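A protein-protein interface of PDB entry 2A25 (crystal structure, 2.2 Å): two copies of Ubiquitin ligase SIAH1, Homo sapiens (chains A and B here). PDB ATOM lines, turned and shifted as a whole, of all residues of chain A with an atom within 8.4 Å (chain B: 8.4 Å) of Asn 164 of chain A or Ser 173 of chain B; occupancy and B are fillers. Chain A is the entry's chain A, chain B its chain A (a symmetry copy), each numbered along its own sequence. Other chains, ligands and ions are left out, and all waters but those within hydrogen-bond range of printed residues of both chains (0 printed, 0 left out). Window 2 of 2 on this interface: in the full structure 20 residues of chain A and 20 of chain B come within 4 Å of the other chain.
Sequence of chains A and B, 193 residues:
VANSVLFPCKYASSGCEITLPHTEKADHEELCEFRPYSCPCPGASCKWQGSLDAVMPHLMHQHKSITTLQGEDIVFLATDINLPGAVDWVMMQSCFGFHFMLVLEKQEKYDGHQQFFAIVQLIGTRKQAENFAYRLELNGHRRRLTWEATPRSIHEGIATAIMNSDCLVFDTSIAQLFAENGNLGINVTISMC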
ATOM      1  N   GLN A 115      -1.973 -11.570  -0.756  1.00  0.00           N
ATOM      2  CA  GLN A 115      -1.418 -12.530   0.195  1.00  0.00           C
ATOM      3  C   GLN A 115      -2.117 -13.885   0.132  1.00  0.00           C
ATOM      4  O   GLN A 115      -3.306 -13.984  -0.177  1.00  0.00           O
ATOM      5  CB  GLN A 115      -1.455 -11.979   1.625  1.00  0.00           C
ATOM      6  CG  GLN A 115      -0.202 -11.164   1.997  1.00  0.00           C
ATOM      7  CD  GLN A 115      -0.106 -10.830   3.489  1.00  0.00           C
ATOM      8  OE1 GLN A 115      -1.080 -10.361   4.099  1.00  0.00           O
ATOM      9  NE2 GLN A 115       1.079 -11.058   4.075  1.00  0.00           N
ATOM     10  N   PHE A 117      -3.099 -17.365   2.265  1.00  0.00           N
ATOM     11  CA  PHE A 117      -3.389 -17.944   3.578  1.00  0.00           C
ATOM     12  C   PHE A 117      -3.611 -19.454   3.451  1.00  0.00           C
ATOM     13  O   PHE A 117      -4.452 -19.864   2.672  1.00  0.00           O
ATOM     14  CB  PHE A 117      -4.615 -17.252   4.197  1.00  0.00           C
ATOM     15  CG  PHE A 117      -4.471 -15.743   4.288  1.00  0.00           C
ATOM     16  CD1 PHE A 117      -4.885 -14.923   3.251  1.00  0.00           C
ATOM     17  CD2 PHE A 117      -3.892 -15.157   5.406  1.00  0.00           C
ATOM     18  CE1 PHE A 117      -4.723 -13.552   3.331  1.00  0.00           C
ATOM     19  CE2 PHE A 117      -3.731 -13.792   5.489  1.00  0.00           C
ATOM     20  CZ  PHE A 117      -4.140 -12.988   4.455  1.00  0.00           C
ATOM     21  N   TRP A 147       4.864 -23.709   9.216  1.00  0.00           N
ATOM     22  CA  TRP A 147       3.871 -23.182  10.166  1.00  0.00           C
ATOM     23  C   TRP A 147       3.287 -24.348  10.931  1.00  0.00           C
ATOM     24  O   TRP A 147       2.878 -25.308  10.321  1.00  0.00           O
ATOM     25  CB  TRP A 147       2.727 -22.478   9.407  1.00  0.00           C
ATOM     26  CG  TRP A 147       1.545 -22.159  10.321  1.00  0.00           C
ATOM     27  CD1 TRP A 147       0.339 -22.844  10.402  1.00  0.00           C
ATOM     28  CD2 TRP A 147       1.448 -21.079  11.251  1.00  0.00           C
ATOM     29  NE1 TRP A 147      -0.475 -22.250  11.339  1.00  0.00           N
ATOM     30  CE2 TRP A 147       0.169 -21.156  11.860  1.00  0.00           C
ATOM     31  CE3 TRP A 147       2.295 -20.020  11.606  1.00  0.00           C
ATOM     32  CZ2 TRP A 147      -0.249 -20.261  12.842  1.00  0.00           C
ATOM     33  CZ3 TRP A 147       1.864 -19.100  12.562  1.00  0.00           C
ATOM     34  CH2 TRP A 147       0.602 -19.244  13.183  1.00  0.00           C
ATOM     35  N   ARG A 152      -8.129 -25.654  13.719  1.00  0.00           N
ATOM     36  CA  ARG A 152      -9.412 -25.075  14.098  1.00  0.00           C
ATOM     37  C   ARG A 152     -10.489 -26.131  13.902  1.00  0.00           C
ATOM     38  O   ARG A 152     -10.362 -26.976  13.035  1.00  0.00           O
ATOM     39  CB  ARG A 152      -9.712 -23.869  13.179  1.00  0.00           C
ATOM     40  CG  ARG A 152      -8.578 -22.750  13.108  1.00  0.00           C
ATOM     41  CD  ARG A 152      -7.989 -22.288  14.479  1.00  0.00           C
ATOM     42  NE  ARG A 152      -8.548 -21.003  14.925  1.00  0.00           N
ATOM     43  CZ  ARG A 152      -7.853 -19.929  15.367  1.00  0.00           C
ATOM     44  NH1 ARG A 152      -6.524 -19.924  15.455  1.00  0.00           N
ATOM     45  NH2 ARG A 152      -8.511 -18.835  15.711  1.00  0.00           N
ATOM     46  N   GLU A 156     -15.359 -23.036  14.595  1.00  0.00           N
ATOM     47  CA  GLU A 156     -14.582 -21.794  14.662  1.00  0.00           C
ATOM     48  C   GLU A 156     -14.505 -21.132  13.298  1.00  0.00           C
ATOM     49  O   GLU A 156     -14.378 -19.911  13.213  1.00  0.00           O
ATOM     50  CB  GLU A 156     -13.168 -22.012  15.233  1.00  0.00           C
ATOM     51  CG  GLU A 156     -12.356 -20.726  15.460  1.00  0.00           C
ATOM     52  CD  GLU A 156     -11.458 -20.356  14.275  1.00  0.00           C
ATOM     53  OE1 GLU A 156     -11.429 -21.116  13.293  1.00  0.00           O
ATOM     54  OE2 GLU A 156     -10.758 -19.321  14.306  1.00  0.00           O
ATOM     55  N   ILE A 158     -12.849 -20.336   9.411  1.00  0.00           N
ATOM     56  CA  ILE A 158     -11.462 -19.952   9.090  1.00  0.00           C
ATOM     57  C   ILE A 158     -11.282 -18.467   8.770  1.00  0.00           C
ATOM     58  O   ILE A 158     -10.153 -17.957   8.786  1.00  0.00           O
ATOM     59  CB  ILE A 158     -10.812 -20.862   7.999  1.00  0.00           C
ATOM     60  CG1 ILE A 158     -11.675 -20.918   6.731  1.00  0.00           C
ATOM     61  CG2 ILE A 158     -10.507 -22.285   8.557  1.00  0.00           C
ATOM     62  CD1 ILE A 158     -11.025 -21.714   5.604  1.00  0.00           C
ATOM     63  N   ALA A 159     -12.390 -17.785   8.494  1.00  0.00           N
ATOM     64  CA  ALA A 159     -12.410 -16.339   8.405  1.00  0.00           C
ATOM     65  C   ALA A 159     -11.693 -15.681   9.593  1.00  0.00           C
ATOM     66  O   ALA A 159     -10.859 -14.824   9.390  1.00  0.00           O
ATOM     67  CB  ALA A 159     -13.830 -15.841   8.303  1.00  0.00           C
ATOM     68  N   THR A 160     -11.992 -16.100  10.819  1.00  0.00           N
ATOM     69  CA  THR A 160     -11.389 -15.460  11.997  1.00  0.00           C
ATOM     70  C   THR A 160      -9.883 -15.721  12.105  1.00  0.00           C
ATOM     71  O   THR A 160      -9.087 -14.786  12.357  1.00  0.00           O
ATOM     72  CB  THR A 160     -12.136 -15.807  13.328  1.00  0.00           C
ATOM     73  OG1 THR A 160     -13.206 -16.724  13.084  1.00  0.00           O
ATOM     74  CG2 THR A 160     -12.886 -14.615  13.816  1.00  0.00           C
ATOM     75  N   ALA A 161      -9.500 -16.982  11.863  1.00  0.00           N
ATOM     76  CA  ALA A 161      -8.084 -17.368  11.829  1.00  0.00           C
ATOM     77  C   ALA A 161      -7.339 -16.651  10.738  1.00  0.00           C
ATOM     78  O   ALA A 161      -6.216 -16.212  10.967  1.00  0.00           O
ATOM     79  CB  ALA A 161      -7.915 -18.854  11.702  1.00  0.00           C
ATOM     80  N   ILE A 162      -7.978 -16.463   9.579  1.00  0.00           N
ATOM     81  CA  ILE A 162      -7.332 -15.799   8.433  1.00  0.00           C
ATOM     82  C   ILE A 162      -7.128 -14.317   8.675  1.00  0.00           C
ATOM     83  O   ILE A 162      -6.094 -13.728   8.303  1.00  0.00           O
ATOM     84  CB  ILE A 162      -8.112 -16.070   7.111  1.00  0.00           C
ATOM     85  CG1 ILE A 162      -7.645 -17.404   6.523  1.00  0.00           C
ATOM     86  CG2 ILE A 162      -7.913 -14.960   6.093  1.00  0.00           C
ATOM     87  CD1 ILE A 162      -8.735 -18.237   5.929  1.00  0.00           C
ATOM     88  N   MET A 163      -8.117 -13.713   9.318  1.00  0.00           N
ATOM     89  CA  MET A 163      -8.096 -12.283   9.509  1.00  0.00           C
ATOM     90  C   MET A 163      -7.005 -11.907  10.550  1.00  0.00           C
ATOM     91  O   MET A 163      -6.404 -10.840  10.463  1.00  0.00           O
ATOM     92  CB  MET A 163      -9.513 -11.778   9.833  1.00  0.00           C
ATOM     93  CG  MET A 163     -10.406 -11.430   8.569  1.00  0.00           C
ATOM     94  SD  MET A 163     -10.898 -12.738   7.291  1.00  0.00           S
ATOM     95  CE  MET A 163     -12.587 -12.166   6.760  1.00  0.00           C
ATOM     96  N   ASN A 164      -6.709 -12.831  11.473  1.00  0.00           N
ATOM     97  CA  ASN A 164      -5.643 -12.659  12.475  1.00  0.00           C
ATOM     98  C   ASN A 164      -4.270 -13.165  11.996  1.00  0.00           C
ATOM     99  O   ASN A 164      -3.330 -13.284  12.805  1.00  0.00           O
ATOM    100  CB  ASN A 164      -5.996 -13.447  13.753  1.00  0.00           C
ATOM    101  CG  ASN A 164      -7.344 -13.071  14.335  1.00  0.00           C
ATOM    102  OD1 ASN A 164      -7.785 -11.942  14.200  1.00  0.00           O
ATOM    103  ND2 ASN A 164      -8.007 -14.029  14.983  1.00  0.00           N
ATOM    104  N   SER A 165      -4.165 -13.534  10.712  1.00  0.00           N
ATOM    105  CA  SER A 165      -2.980 -14.230  10.187  1.00  0.00           C
ATOM    106  C   SER A 165      -2.569 -15.449  11.047  1.00  0.00           C
ATOM    107  O   SER A 165      -1.375 -15.771  11.162  1.00  0.00           O
ATOM    108  CB  SER A 165      -1.781 -13.280  10.046  1.00  0.00           C
ATOM    109  OG  SER A 165      -2.102 -12.079   9.366  1.00  0.00           O
ATOM    110  N   ASP A 166      -3.565 -16.100  11.656  1.00  0.00           N
ATOM    111  CA  ASP A 166      -3.372 -17.343  12.427  1.00  0.00           C
ATOM    112  C   ASP A 166      -3.320 -18.614  11.560  1.00  0.00           C
ATOM    113  O   ASP A 166      -4.158 -19.529  11.672  1.00  0.00           O
ATOM    114  CB  ASP A 166      -4.459 -17.480  13.485  1.00  0.00           C
ATOM    115  CG  ASP A 166      -3.923 -18.027  14.792  1.00  0.00           C
ATOM    116  OD1 ASP A 166      -2.812 -18.610  14.798  1.00  0.00           O
ATOM    117  OD2 ASP A 166      -4.556 -17.925  15.866  1.00  0.00           O
ATOM    118  N   CYS A 167      -2.304 -18.671  10.704  1.00  0.00           N
ATOM    119  CA  CYS A 167      -2.183 -19.730   9.718  1.00  0.00           C
ATOM    120  C   CYS A 167      -0.897 -19.419   9.000  1.00  0.00           C
ATOM    121  O   CYS A 167      -0.178 -18.492   9.379  1.00  0.00           O
ATOM    122  CB  CYS A 167      -3.359 -19.692   8.743  1.00  0.00           C
ATOM    123  SG  CYS A 167      -3.670 -18.056   8.012  1.00  0.00           S
ATOM    124  N   VAL A 169       0.950 -17.589   6.370  1.00  0.00           N
ATOM    125  CA  VAL A 169       0.733 -16.386   5.608  1.00  0.00           C
ATOM    126  C   VAL A 169       2.002 -16.125   4.830  1.00  0.00           C
ATOM    127  O   VAL A 169       3.107 -16.049   5.396  1.00  0.00           O
ATOM    128  CB  VAL A 169       0.402 -15.199   6.516  1.00  0.00           C
ATOM    129  CG1 VAL A 169       0.360 -13.886   5.725  1.00  0.00           C
ATOM    130  CG2 VAL A 169      -0.915 -15.445   7.214  1.00  0.00           C
ATOM    131  N   ILE B  81       8.652  -3.584  19.870  1.00  0.00           N
ATOM    132  CA  ILE B  81       8.328  -3.692  18.443  1.00  0.00           C
ATOM    133  C   ILE B  81       7.234  -2.743  17.910  1.00  0.00           C
ATOM    134  O   ILE B  81       6.858  -2.839  16.742  1.00  0.00           O
ATOM    135  CB  ILE B  81       8.096  -5.174  18.019  1.00  0.00           C
ATOM    136  CG1 ILE B  81       7.011  -5.855  18.859  1.00  0.00           C
ATOM    137  CG2 ILE B  81       9.409  -5.952  18.088  1.00  0.00           C
ATOM    138  CD1 ILE B  81       6.714  -7.305  18.401  1.00  0.00           C
ATOM    139  N   GLN B 114       2.306  -2.511   8.537  1.00  0.00           N
ATOM    140  CA  GLN B 114       3.747  -2.728   8.620  1.00  0.00           C
ATOM    141  C   GLN B 114       4.088  -4.213   8.560  1.00  0.00           C
ATOM    142  O   GLN B 114       3.302  -5.043   9.016  1.00  0.00           O
ATOM    143  CB  GLN B 114       4.321  -2.141   9.913  1.00  0.00           C
ATOM    144  CG  GLN B 114       3.488  -1.016  10.517  1.00  0.00           C
ATOM    145  CD  GLN B 114       3.869  -0.728  11.956  1.00  0.00           C
ATOM    146  OE1 GLN B 114       3.519  -1.490  12.864  1.00  0.00           O
ATOM    147  NE2 GLN B 114       4.587   0.372  12.169  1.00  0.00           N
ATOM    148  N   GLN B 115       5.265  -4.525   8.012  1.00  0.00           N
ATOM    149  CA  GLN B 115       5.800  -5.884   8.024  1.00  0.00           C
ATOM    150  C   GLN B 115       7.174  -5.964   8.684  1.00  0.00           C
ATOM    151  O   GLN B 115       7.966  -5.022   8.643  1.00  0.00           O
ATOM    152  CB  GLN B 115       5.855  -6.472   6.610  1.00  0.00           C
ATOM    153  CG  GLN B 115       4.554  -7.184   6.195  1.00  0.00           C
ATOM    154  CD  GLN B 115       4.681  -7.994   4.901  1.00  0.00           C
ATOM    155  OE1 GLN B 115       5.202  -7.497   3.889  1.00  0.00           O
ATOM    156  NE2 GLN B 115       4.190  -9.242   4.929  1.00  0.00           N
ATOM    157  N   PHE B 116       7.421  -7.107   9.301  1.00  0.00           N
ATOM    158  CA  PHE B 116       8.700  -7.438   9.885  1.00  0.00           C
ATOM    159  C   PHE B 116       9.486  -8.368   8.980  1.00  0.00           C
ATOM    160  O   PHE B 116       8.932  -9.325   8.415  1.00  0.00           O
ATOM    161  CB  PHE B 116       8.488  -8.120  11.224  1.00  0.00           C
ATOM    162  CG  PHE B 116       8.043  -7.190  12.297  1.00  0.00           C
ATOM    163  CD1 PHE B 116       6.685  -6.925  12.489  1.00  0.00           C
ATOM    164  CD2 PHE B 116       8.972  -6.546  13.106  1.00  0.00           C
ATOM    165  CE1 PHE B 116       6.271  -6.033  13.482  1.00  0.00           C
ATOM    166  CE2 PHE B 116       8.560  -5.669  14.106  1.00  0.00           C
ATOM    167  CZ  PHE B 116       7.207  -5.419  14.290  1.00  0.00           C
ATOM    168  N   ARG B 143       1.574 -22.328  18.633  1.00  0.00           N
ATOM    169  CA  ARG B 143       1.847 -21.841  17.278  1.00  0.00           C
ATOM    170  C   ARG B 143       3.345 -21.757  17.106  1.00  0.00           C
ATOM    171  O   ARG B 143       4.052 -21.371  18.040  1.00  0.00           O
ATOM    172  CB  ARG B 143       1.303 -20.431  17.105  1.00  0.00           C
ATOM    173  CG  ARG B 143      -0.188 -20.333  17.147  1.00  0.00           C
ATOM    174  CD  ARG B 143      -0.669 -18.924  17.338  1.00  0.00           C
ATOM    175  NE  ARG B 143      -2.127 -18.817  17.343  1.00  0.00           N
ATOM    176  CZ  ARG B 143      -2.886 -18.920  18.431  1.00  0.00           C
ATOM    177  NH1 ARG B 143      -2.336 -19.160  19.615  1.00  0.00           N
ATOM    178  NH2 ARG B 143      -4.197 -18.800  18.340  1.00  0.00           N
ATOM    179  N   PHE B 170       6.832 -11.570   8.492  1.00  0.00           N
ATOM    180  CA  PHE B 170       5.600 -11.678   9.226  1.00  0.00           C
ATOM    181  C   PHE B 170       5.104 -10.280   9.489  1.00  0.00           C
ATOM    182  O   PHE B 170       5.886  -9.333   9.562  1.00  0.00           O
ATOM    183  CB  PHE B 170       5.788 -12.456  10.529  1.00  0.00           C
ATOM    184  CG  PHE B 170       6.931 -11.972  11.377  1.00  0.00           C
ATOM    185  CD1 PHE B 170       6.688 -11.189  12.506  1.00  0.00           C
ATOM    186  CD2 PHE B 170       8.255 -12.299  11.057  1.00  0.00           C
ATOM    187  CE1 PHE B 170       7.744 -10.757  13.307  1.00  0.00           C
ATOM    188  CE2 PHE B 170       9.299 -11.856  11.823  1.00  0.00           C
ATOM    189  CZ  PHE B 170       9.040 -11.084  12.961  1.00  0.00           C
ATOM    190  N   ASP B 171       3.798 -10.146   9.609  1.00  0.00           N
ATOM    191  CA  ASP B 171       3.212  -8.828   9.806  1.00  0.00           C
ATOM    192  C   ASP B 171       2.898  -8.577  11.289  1.00  0.00           C
ATOM    193  O   ASP B 171       3.150  -9.461  12.130  1.00  0.00           O
ATOM    194  CB  ASP B 171       2.012  -8.639   8.881  1.00  0.00           C
ATOM    195  CG  ASP B 171       1.031  -9.786   8.946  1.00  0.00           C
ATOM    196  OD1 ASP B 171       0.447  -9.990  10.048  1.00  0.00           O
ATOM    197  OD2 ASP B 171       0.765 -10.510   7.942  1.00  0.00           O
ATOM    198  N   THR B 172       2.382  -7.386  11.613  1.00  0.00           N
ATOM    199  CA  THR B 172       2.214  -6.999  13.011  1.00  0.00           C
ATOM    200  C   THR B 172       1.303  -7.930  13.805  1.00  0.00           C
ATOM    201  O   THR B 172       1.652  -8.310  14.924  1.00  0.00           O
ATOM    202  CB  THR B 172       1.742  -5.515  13.199  1.00  0.00           C
ATOM    203  OG1 THR B 172       1.570  -4.871  11.931  1.00  0.00           O
ATOM    204  CG2 THR B 172       2.847  -4.713  13.864  1.00  0.00           C
ATOM    205  N   SER B 173       0.153  -8.297  13.237  1.00  0.00           N
ATOM    206  CA  SER B 173      -0.781  -9.167  13.948  1.00  0.00           C
ATOM    207  C   SER B 173      -0.069 -10.440  14.397  1.00  0.00           C
ATOM    208  O   SER B 173      -0.154 -10.800  15.575  1.00  0.00           O
ATOM    209  CB  SER B 173      -2.063  -9.447  13.133  1.00  0.00           C
ATOM    210  OG  SER B 173      -1.821 -10.389  12.094  1.00  0.00           O
ATOM    211  N   ILE B 174       0.662 -11.073  13.474  1.00  0.00           N
ATOM    212  CA  ILE B 174       1.583 -12.184  13.783  1.00  0.00           C
ATOM    213  C   ILE B 174       2.654 -11.810  14.832  1.00  0.00           C
ATOM    214  O   ILE B 174       2.904 -12.573  15.766  1.00  0.00           O
ATOM    215  CB  ILE B 174       2.271 -12.722  12.488  1.00  0.00           C
ATOM    216  CG1 ILE B 174       1.284 -13.439  11.586  1.00  0.00           C
ATOM    217  CG2 ILE B 174       3.419 -13.715  12.802  1.00  0.00           C
ATOM    218  CD1 ILE B 174       1.873 -13.774  10.199  1.00  0.00           C
ATOM    219  N   ALA B 175       3.300 -10.662  14.670  1.00  0.00           N
ATOM    220  CA  ALA B 175       4.313 -10.245  15.643  1.00  0.00           C
ATOM    221  C   ALA B 175       3.711 -10.180  17.060  1.00  0.00           C
ATOM    222  O   ALA B 175       4.254 -10.763  17.995  1.00  0.00           O
ATOM    223  CB  ALA B 175       4.945  -8.919  15.238  1.00  0.00           C
ATOM    224  N   GLN B 176       2.562  -9.514  17.185  1.00  0.00           N
ATOM    225  CA  GLN B 176       1.794  -9.417  18.436  1.00  0.00           C
ATOM    226  C   GLN B 176       1.503 -10.809  19.043  1.00  0.00           C
ATOM    227  O   GLN B 176       1.576 -11.013  20.261  1.00  0.00           O
ATOM    228  CB  GLN B 176       0.489  -8.652  18.151  1.00  0.00           C
ATOM    229  CG  GLN B 176      -0.487  -8.529  19.309  1.00  0.00           C
ATOM    230  CD  GLN B 176      -1.983  -8.592  18.892  1.00  0.00           C
ATOM    231  OE1 GLN B 176      -2.836  -8.001  19.577  1.00  0.00           O
ATOM    232  NE2 GLN B 176      -2.296  -9.307  17.793  1.00  0.00           N
ATOM    233  N   LEU B 177       1.190 -11.751  18.161  1.00  0.00           N
ATOM    234  CA  LEU B 177       0.833 -13.128  18.493  1.00  0.00           C
ATOM    235  C   LEU B 177       1.957 -13.965  19.145  1.00  0.00           C
ATOM    236  O   LEU B 177       1.674 -14.832  19.987  1.00  0.00           O
ATOM    237  CB  LEU B 177       0.379 -13.812  17.199  1.00  0.00           C
ATOM    238  CG  LEU B 177      -0.271 -15.191  17.163  1.00  0.00           C
ATOM    239  CD1 LEU B 177      -1.692 -15.120  17.671  1.00  0.00           C
ATOM    240  CD2 LEU B 177      -0.222 -15.730  15.719  1.00  0.00           C
ATOM    241  N   PHE B 178       3.204 -13.730  18.734  1.00  0.00           N
ATOM    242  CA  PHE B 178       4.360 -14.458  19.263  1.00  0.00           C
ATOM    243  C   PHE B 178       5.070 -13.690  20.380  1.00  0.00           C
ATOM    244  O   PHE B 178       5.871 -14.266  21.130  1.00  0.00           O
ATOM    245  CB  PHE B 178       5.355 -14.778  18.138  1.00  0.00           C
ATOM    246  CG  PHE B 178       4.856 -15.821  17.179  1.00  0.00           C
ATOM    247  CD1 PHE B 178       4.453 -15.471  15.895  1.00  0.00           C
ATOM    248  CD2 PHE B 178       4.748 -17.154  17.573  1.00  0.00           C
ATOM    249  CE1 PHE B 178       3.957 -16.437  15.012  1.00  0.00           C
ATOM    250  CE2 PHE B 178       4.277 -18.129  16.695  1.00  0.00           C
ATOM    251  CZ  PHE B 178       3.876 -17.769  15.409  1.00  0.00           C
ATOM    252  N   ALA B 179       4.748 -12.400  20.485  1.00  0.00           N
ATOM    253  CA  ALA B 179       5.430 -11.475  21.381  1.00  0.00           C
ATOM    254  C   ALA B 179       4.825 -11.379  22.777  1.00  0.00           C
ATOM    255  O   ALA B 179       3.606 -11.566  22.968  1.00  0.00           O
ATOM    256  CB  ALA B 179       5.501 -10.096  20.749  1.00  0.00           C
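The side-chain carboxylate (OD1) of Asp 166 of chain A is in salt-bridge range of the guanidinium group (NE) of Arg 143 of chain B, 2.6 Å away.
OG of Ser 165 of chain A is in hydrogen-bond range of OG of Ser 173 of chain B (3.2 Å).
The backbone carbonyl oxygen (O) of Asn 164 of chain A lies within hydrogen-bond range of the side-chain hydroxyl (OG) of Ser 173 of chain B.
The side-chain hydroxyl (OG) of Ser 165 of chain A lies within hydrogen-bond range of the side-chain carboxylate (OD1) of Asp 171 of chain B (3.4 Å).
The side-chain carboxylate of Glu 156 of chain A is in salt-bridge range of the guanidinium group of Arg 152 of chain A.
The backbone carbonyl oxygen of Thr 160 of chain A sits at hydrogen-bond distance from the side-chain amide nitrogen of Asn 164 of chain A, 2.9 Å away.
O of Ser 173 of chain B sits close to NE2 of Gln 176 of chain B (3.4 Å).
The side-chain hydroxyl (OG) of Ser 173 of chain B is in hydrogen-bond range of the side-chain carboxylate (OD1) of Asp 171 of chain B (3.1 Å).
The backbone carbonyl oxygen (O) of Ala 161 of chain A lies within hydrogen-bond range of the backbone NH (N) of Asp 166 of chain A (2.7 Å).
The guanidinium group (NH1) of Arg 152 of chain A lies within salt-bridge range of the side-chain carboxylate (OD2) of Asp 166 of chain A (2.8 Å).
NE2 of Gln 115 of chain A touches NE2 of Gln 115 of chain B, 3.7 Å away.
OD2 of Asp 171 of chain B touches NE2 of Gln 115 of chain A, at 3.9 Å.
Trp 147 of chain A touches Phe 178 of chain B.
Arg 152 of chain A touches Arg 143 of chain B (NH1 to NH2, 3.9 Å).
Ile 174 of chain B touches Ser 165 of chain A (CG1 to CB, 3.4 Å).
Leu 177 of chain B touches Asp 166 of chain A.
Of the printed residues of chain B, Trp 147 of chain A touches Phe 178.
Ser 165 of chain A touches just these residues of chain B: Asp 171 (3.4 Å), Ser 173 (3.2 Å) and Ile 174 (3.4 Å).
Ser 173 of chain B touches just these residues of chain A: Asn 164 and Ser 165.
Of the printed residues of chain A, Ile 174 of chain B touches Ser 165 (3.4 Å).
The nearest residue of chain A that does not touch Ser 173 of chain B is Met 163 of chain A (4.9 Å).
Of the 16 printed residues of chain A, 6 touch a printed residue of chain B.
Printed residues of chain A that touch a printed residue of chain B: Gln 115, Trp 147, Arg 152, Asn 164, Ser 165 and Asp 166.
Hydrophobic or aromatic side chains of chain A that line the printed part of chain B: Trp 147.
Of the 15 printed residues of chain B, 7 touch a printed residue of chain A.
Hydrophobic or aromatic side chains of chain B that line the printed part of chain A: Ile 174, Leu 177 and Phe 178.
Among the printed residues, Asp or Glu carboxylates within 4 Å of a Lys or Arg side-chain nitrogen of the other chain: Asp 166 of chain A with Arg 143 of chain B (2.6 Å).
Gln 115 of chain B touches its own counterpart, Gln 115 of chain A.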
